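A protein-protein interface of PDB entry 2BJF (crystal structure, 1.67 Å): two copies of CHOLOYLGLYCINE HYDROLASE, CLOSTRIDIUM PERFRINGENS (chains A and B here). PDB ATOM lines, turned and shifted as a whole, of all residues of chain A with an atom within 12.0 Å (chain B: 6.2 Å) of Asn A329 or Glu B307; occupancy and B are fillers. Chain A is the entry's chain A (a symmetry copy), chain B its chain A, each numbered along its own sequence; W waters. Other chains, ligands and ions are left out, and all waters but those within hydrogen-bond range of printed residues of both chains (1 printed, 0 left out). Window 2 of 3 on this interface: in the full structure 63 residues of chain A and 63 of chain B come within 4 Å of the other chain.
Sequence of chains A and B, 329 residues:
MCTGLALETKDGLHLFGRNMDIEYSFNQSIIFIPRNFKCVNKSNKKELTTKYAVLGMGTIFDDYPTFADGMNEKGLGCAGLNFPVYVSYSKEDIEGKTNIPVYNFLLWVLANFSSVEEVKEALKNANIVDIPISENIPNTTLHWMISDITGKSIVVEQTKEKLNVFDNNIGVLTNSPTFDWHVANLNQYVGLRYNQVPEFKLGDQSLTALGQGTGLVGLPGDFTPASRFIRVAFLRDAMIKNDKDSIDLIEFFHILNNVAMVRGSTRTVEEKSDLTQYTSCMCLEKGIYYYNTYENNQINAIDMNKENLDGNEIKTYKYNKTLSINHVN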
ATOM      1  N   ILE A 325     -31.648  28.355 -19.692  1.00  0.00           N
ATOM      2  CA  ILE A 325     -30.223  28.073 -19.848  1.00  0.00           C
ATOM      3  C   ILE A 325     -29.511  29.286 -20.441  1.00  0.00           C
ATOM      4  O   ILE A 325     -30.027  29.934 -21.355  1.00  0.00           O
ATOM      5  CB  ILE A 325     -29.992  26.823 -20.745  1.00  0.00           C
ATOM      6  CG1 ILE A 325     -30.592  25.574 -20.088  1.00  0.00           C
ATOM      7  CG2 ILE A 325     -28.500  26.615 -21.037  1.00  0.00           C
ATOM      8  CD1 ILE A 325     -30.703  24.365 -21.012  1.00  0.00           C
ATOM      9  N   ASN A 326     -28.335  29.598 -19.900  1.00  0.00           N
ATOM     10  CA  ASN A 326     -27.475  30.621 -20.477  1.00  0.00           C
ATOM     11  C   ASN A 326     -26.550  29.996 -21.516  1.00  0.00           C
ATOM     12  O   ASN A 326     -25.610  29.275 -21.172  1.00  0.00           O
ATOM     13  CB  ASN A 326     -26.665  31.338 -19.390  1.00  0.00           C
ATOM     14  CG  ASN A 326     -25.690  32.355 -19.963  1.00  0.00           C
ATOM     15  OD1 ASN A 326     -26.036  33.138 -20.850  1.00  0.00           O
ATOM     16  ND2 ASN A 326     -24.464  32.349 -19.453  1.00  0.00           N
ATOM     17  N   HIS A 327     -26.835  30.264 -22.787  1.00  0.00           N
ATOM     18  CA  HIS A 327     -26.023  29.742 -23.880  1.00  0.00           C
ATOM     19  C   HIS A 327     -24.835  30.663 -24.129  1.00  0.00           C
ATOM     20  O   HIS A 327     -24.991  31.803 -24.571  1.00  0.00           O
ATOM     21  CB  HIS A 327     -26.872  29.540 -25.136  1.00  0.00           C
ATOM     22  CG  HIS A 327     -27.974  28.542 -24.953  1.00  0.00           C
ATOM     23  ND1 HIS A 327     -27.770  27.183 -25.044  1.00  0.00           N
ATOM     24  CD2 HIS A 327     -29.288  28.706 -24.664  1.00  0.00           C
ATOM     25  CE1 HIS A 327     -28.911  26.552 -24.828  1.00  0.00           C
ATOM     26  NE2 HIS A 327     -29.847  27.454 -24.596  1.00  0.00           N
ATOM     27  N   VAL A 328     -23.649  30.142 -23.825  1.00  0.00           N
ATOM     28  CA  VAL A 328     -22.418  30.925 -23.766  1.00  0.00           C
ATOM     29  C   VAL A 328     -21.794  31.139 -25.148  1.00  0.00           C
ATOM     30  O   VAL A 328     -21.229  32.202 -25.424  1.00  0.00           O
ATOM     31  CB  VAL A 328     -21.392  30.260 -22.805  1.00  0.00           C
ATOM     32  CG1 VAL A 328     -20.136  31.100 -22.670  1.00  0.00           C
ATOM     33  CG2 VAL A 328     -22.023  30.029 -21.431  1.00  0.00           C
ATOM     34  N   ASN A 329     -21.905  30.135 -26.013  1.00  0.00           N
ATOM     35  CA  ASN A 329     -21.294  30.195 -27.338  1.00  0.00           C
ATOM     36  C   ASN A 329     -22.250  29.800 -28.463  1.00  0.00           C
ATOM     37  O   ASN A 329     -23.464  29.715 -28.270  1.00  0.00           O
ATOM     38  CB  ASN A 329     -20.013  29.347 -27.376  1.00  0.00           C
ATOM     39  CG  ASN A 329     -20.289  27.850 -27.461  1.00  0.00           C
ATOM     40  OD1 ASN A 329     -21.327  27.362 -27.011  1.00  0.00           O
ATOM     41  ND2 ASN A 329     -19.348  27.115 -28.043  1.00  0.00           N
ATOM     42  OXT ASN A 329     -21.830  29.554 -29.592  1.00  0.00           O
ATOM     43  N   PHE B  32     -11.469  24.466 -24.423  1.00  0.00           N
ATOM     44  CA  PHE B  32     -11.647  23.778 -25.696  1.00  0.00           C
ATOM     45  C   PHE B  32     -10.300  23.608 -26.390  1.00  0.00           C
ATOM     46  O   PHE B  32      -9.553  24.577 -26.555  1.00  0.00           O
ATOM     47  CB  PHE B  32     -12.614  24.548 -26.607  1.00  0.00           C
ATOM     48  CG  PHE B  32     -12.687  24.008 -28.014  1.00  0.00           C
ATOM     49  CD1 PHE B  32     -13.475  22.898 -28.307  1.00  0.00           C
ATOM     50  CD2 PHE B  32     -11.966  24.609 -29.044  1.00  0.00           C
ATOM     51  CE1 PHE B  32     -13.545  22.392 -29.603  1.00  0.00           C
ATOM     52  CE2 PHE B  32     -12.026  24.108 -30.345  1.00  0.00           C
ATOM     53  CZ  PHE B  32     -12.819  22.998 -30.625  1.00  0.00           C
ATOM     54  N   ALA B 301     -24.301  26.730 -20.844  1.00  0.00           N
ATOM     55  CA  ALA B 301     -24.035  25.741 -21.887  1.00  0.00           C
ATOM     56  C   ALA B 301     -22.942  26.192 -22.847  1.00  0.00           C
ATOM     57  O   ALA B 301     -22.974  27.313 -23.357  1.00  0.00           O
ATOM     58  CB  ALA B 301     -25.312  25.426 -22.654  1.00  0.00           C
ATOM     59  N   ILE B 302     -21.974  25.309 -23.076  1.00  0.00           N
ATOM     60  CA  ILE B 302     -20.940  25.516 -24.089  1.00  0.00           C
ATOM     61  C   ILE B 302     -20.962  24.323 -25.040  1.00  0.00           C
ATOM     62  O   ILE B 302     -20.754  23.180 -24.625  1.00  0.00           O
ATOM     63  CB  ILE B 302     -19.536  25.715 -23.458  1.00  0.00           C
ATOM     64  CG1 ILE B 302     -19.506  27.014 -22.647  1.00  0.00           C
ATOM     65  CG2 ILE B 302     -18.450  25.751 -24.539  1.00  0.00           C
ATOM     66  CD1 ILE B 302     -18.589  26.992 -21.451  1.00  0.00           C
ATOM     67  N   ASP B 303     -21.236  24.605 -26.311  1.00  0.00           N
ATOM     68  CA  ASP B 303     -21.359  23.585 -27.346  1.00  0.00           C
ATOM     69  C   ASP B 303     -20.056  23.515 -28.135  1.00  0.00           C
ATOM     70  O   ASP B 303     -19.710  24.451 -28.861  1.00  0.00           O
ATOM     71  CB  ASP B 303     -22.542  23.929 -28.266  1.00  0.00           C
ATOM     72  CG  ASP B 303     -22.873  22.825 -29.267  1.00  0.00           C
ATOM     73  OD1 ASP B 303     -22.030  21.935 -29.519  1.00  0.00           O
ATOM     74  OD2 ASP B 303     -23.996  22.858 -29.816  1.00  0.00           O
ATOM     75  N   MET B 304     -19.334  22.404 -27.990  1.00  0.00           N
ATOM     76  CA  MET B 304     -18.045  22.237 -28.669  1.00  0.00           C
ATOM     77  C   MET B 304     -18.190  22.190 -30.192  1.00  0.00           C
ATOM     78  O   MET B 304     -17.271  22.572 -30.921  1.00  0.00           O
ATOM     79  CB  MET B 304     -17.296  21.001 -28.149  1.00  0.00           C
ATOM     80  CG  MET B 304     -17.794  19.659 -28.677  1.00  0.00           C
ATOM     81  SD  MET B 304     -16.926  18.246 -27.967  1.00  0.00           S
ATOM     82  CE  MET B 304     -15.251  18.544 -28.524  1.00  0.00           C
ATOM     83  N   ASN B 305     -19.351  21.737 -30.661  1.00  0.00           N
ATOM     84  CA  ASN B 305     -19.611  21.601 -32.094  1.00  0.00           C
ATOM     85  C   ASN B 305     -19.871  22.928 -32.806  1.00  0.00           C
ATOM     86  O   ASN B 305     -19.900  22.986 -34.039  1.00  0.00           O
ATOM     87  CB  ASN B 305     -20.749  20.608 -32.337  1.00  0.00           C
ATOM     88  CG  ASN B 305     -20.331  19.176 -32.066  1.00  0.00           C
ATOM     89  OD1 ASN B 305     -19.430  18.644 -32.720  1.00  0.00           O
ATOM     90  ND2 ASN B 305     -20.983  18.542 -31.099  1.00  0.00           N
ATOM     91  N   LYS B 306     -20.054  23.989 -32.024  1.00  0.00           N
ATOM     92  CA  LYS B 306     -20.163  25.339 -32.569  1.00  0.00           C
ATOM     93  C   LYS B 306     -18.779  25.933 -32.830  1.00  0.00           C
ATOM     94  O   LYS B 306     -18.636  26.846 -33.641  1.00  0.00           O
ATOM     95  CB  LYS B 306     -20.979  26.239 -31.638  1.00  0.00           C
ATOM     96  CG  LYS B 306     -22.443  25.824 -31.526  1.00  0.00           C
ATOM     97  CD  LYS B 306     -23.276  26.847 -30.779  1.00  0.00           C
ATOM     98  CE  LYS B 306     -23.753  27.969 -31.698  1.00  0.00           C
ATOM     99  NZ  LYS B 306     -24.486  29.012 -30.934  1.00  0.00           N
ATOM    100  N   GLU B 307     -17.768  25.400 -32.147  1.00  0.00           N
ATOM    101  CA  GLU B 307     -16.382  25.824 -32.347  1.00  0.00           C
ATOM    102  C   GLU B 307     -15.758  25.131 -33.557  1.00  0.00           C
ATOM    103  O   GLU B 307     -16.291  24.139 -34.061  1.00  0.00           O
ATOM    104  CB  GLU B 307     -15.541  25.543 -31.092  1.00  0.00           C
ATOM    105  CG  GLU B 307     -16.062  26.185 -29.801  1.00  0.00           C
ATOM    106  CD  GLU B 307     -16.096  27.707 -29.842  1.00  0.00           C
ATOM    107  OE1 GLU B 307     -15.210  28.323 -30.478  1.00  0.00           O
ATOM    108  OE2 GLU B 307     -17.013  28.291 -29.228  1.00  0.00           O
ATOM    109  N   ASN B 308     -14.632  25.664 -34.026  1.00  0.00           N
ATOM    110  CA  ASN B 308     -13.886  25.027 -35.106  1.00  0.00           C
ATOM    111  C   ASN B 308     -13.047  23.876 -34.569  1.00  0.00           C
ATOM    112  O   ASN B 308     -12.036  24.092 -33.894  1.00  0.00           O
ATOM    113  CB  ASN B 308     -13.001  26.036 -35.846  1.00  0.00           C
ATOM    114  CG  ASN B 308     -12.485  25.501 -37.178  1.00  0.00           C
ATOM    115  OD1 ASN B 308     -12.727  24.347 -37.538  1.00  0.00           O
ATOM    116  ND2 ASN B 308     -11.771  26.345 -37.916  1.00  0.00           N
ATOM    117  N   LEU B 309     -13.474  22.654 -34.873  1.00  0.00           N
ATOM    118  CA  LEU B 309     -12.742  21.460 -34.456  1.00  0.00           C
ATOM    119  C   LEU B 309     -11.401  21.347 -35.182  1.00  0.00           C
ATOM    120  O   LEU B 309     -10.491  20.669 -34.708  1.00  0.00           O
ATOM    121  CB  LEU B 309     -13.582  20.192 -34.657  1.00  0.00           C
ATOM    122  CG  LEU B 309     -14.988  20.116 -34.040  1.00  0.00           C
ATOM    123  CD1 LEU B 309     -15.555  18.711 -34.198  1.00  0.00           C
ATOM    124  CD2 LEU B 309     -15.026  20.540 -32.571  1.00  0.00           C
ATOM    125  N   ASP B 310     -11.291  22.025 -36.326  1.00  0.00           N
ATOM    126  CA  ASP B 310     -10.047  22.090 -37.094  1.00  0.00           C
ATOM    127  C   ASP B 310      -9.270  23.384 -36.820  1.00  0.00           C
ATOM    128  O   ASP B 310      -8.422  23.790 -37.622  1.00  0.00           O
ATOM    129  CB  ASP B 310     -10.334  21.957 -38.595  1.00  0.00           C
ATOM    130  CG  ASP B 310     -10.902  20.598 -38.969  1.00  0.00           C
ATOM    131  OD1 ASP B 310     -10.418  19.570 -38.446  1.00  0.00           O
ATOM    132  OD2 ASP B 310     -11.830  20.559 -39.805  1.00  0.00           O
ATOM    133  N   LYS B 315      -9.108  27.491 -26.880  1.00  0.00           N
ATOM    134  CA  LYS B 315     -10.110  28.503 -26.560  1.00  0.00           C
ATOM    135  C   LYS B 315     -10.646  28.250 -25.154  1.00  0.00           C
ATOM    136  O   LYS B 315     -10.999  27.119 -24.819  1.00  0.00           O
ATOM    137  CB  LYS B 315     -11.252  28.464 -27.587  1.00  0.00           C
ATOM    138  CG  LYS B 315     -12.449  29.364 -27.276  1.00  0.00           C
ATOM    139  CD  LYS B 315     -12.158  30.830 -27.563  1.00  0.00           C
ATOM    140  CE  LYS B 315     -13.281  31.722 -27.057  1.00  0.00           C
ATOM    141  NZ  LYS B 315     -13.102  33.140 -27.480  1.00  0.00           N
ATOM    142  N   TYR B 317     -13.376  29.577 -21.924  1.00  0.00           N
ATOM    143  CA  TYR B 317     -14.561  30.331 -21.527  1.00  0.00           C
ATOM    144  C   TYR B 317     -14.572  30.539 -20.014  1.00  0.00           C
ATOM    145  O   TYR B 317     -14.228  29.633 -19.250  1.00  0.00           O
ATOM    146  CB  TYR B 317     -15.838  29.626 -21.998  1.00  0.00           C
ATOM    147  CG  TYR B 317     -16.111  29.797 -23.480  1.00  0.00           C
ATOM    148  CD1 TYR B 317     -16.743  30.942 -23.962  1.00  0.00           C
ATOM    149  CD2 TYR B 317     -15.733  28.817 -24.398  1.00  0.00           C
ATOM    150  CE1 TYR B 317     -16.993  31.112 -25.323  1.00  0.00           C
ATOM    151  CE2 TYR B 317     -15.980  28.974 -25.761  1.00  0.00           C
ATOM    152  CZ  TYR B 317     -16.611  30.124 -26.216  1.00  0.00           C
ATOM    153  OH  TYR B 317     -16.855  30.290 -27.560  1.00  0.00           O
HETATM  154  O   HOH W   1     -23.976  27.653 -26.021  1.00  0.00           O
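Ala B301 touches Ile A325. ND1 of His A327 touches CB of Ala B301, 3.9 Å away. CB of Val A328 touches CG1 of Ile B302 (3.8 Å). Val A328 touches Tyr B317. CA of Ile B302 touches OD1 of Asn A329, 3.5 Å away. Tyr B317 touches Asn A329.
No position is printed for both chains. Of the 11 pairs that touch across the chains among the printed residues, none has its exchanged pair printed and touching as well.
The backbone NH of Ala B301 lies within hydrogen-bond range of the backbone carbonyl oxygen of Asn A326, at 2.9 Å. The backbone carbonyl oxygen (O) of Ala B301 is in hydrogen-bond range of the backbone NH (N) of Val A328, at 2.9 Å. The backbone carbonyl oxygen (O) of Asp B303 lies within hydrogen-bond range of the side-chain amide nitrogen (ND2) of Asn A329 (2.8 Å). The side-chain amino group of Lys B306 is in salt-bridge range of the chain-end carboxylate of Asn A329, 2.9 Å away. The side-chain carboxylate (OE2) of Glu B307 sits at hydrogen-bond distance from the side-chain amide nitrogen (ND2) of Asn A329, at 2.9 Å.
Of the 5 printed residues of chain A, 5 touch a printed residue of chain B. Hydrophobic or aromatic side chains of chain A within 4 Å of the printed part of chain B: Ile A325, His A327 and Val A328. Printed residues of chain B that touch a printed residue of chain A: Ala B301, Ile B302, Asp B303, Lys B306, Glu B307 and Tyr B317. Along chain B the printed residues that touch a printed residue of chain A span positions 301 to 317. Among the printed residues, 11 pairs touch across the chains.
Of the printed residues of chain B, Ile A325 touches Ala B301. No residue of chain A comes within 4 Å of Phe B32. Printed residues of chain A within 4 Å of Ala B301: Ile A325 (3.8 Å), Asn A326 (2.9 Å), His A327 (3.9 Å) and Val A328 (2.9 Å). Ile B302 touches just these residues of chain A: Val A328 and Asn A329. Of chain A, only Asn A329 (2.8 Å) comes within 4 Å of Asp B303. No residue of chain A comes within 4 Å of Asn B305. Of the printed residues of chain A, Lys B306 touches Asn A329 (2.9 Å). Glu B307 touches just one residue of chain A: Asn A329 (2.9 Å). No residue of chain A comes within 4 Å of Asn B308. The nearest residue of chain A that does not touch Glu B307 is Val A328 (6.9 Å).
OD1 of Asp B303 lies within hydrogen-bond range of N of Asn B305 (2.9 Å). The side-chain hydroxyl (OH) of Tyr B317 lies within hydrogen-bond range of the side-chain carboxylate (OE2) of Glu B307 (2.6 Å).
Water W1 lies within hydrogen-bond range of OD1 of Asn A329, O of Ala B301 and N of Val A328.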
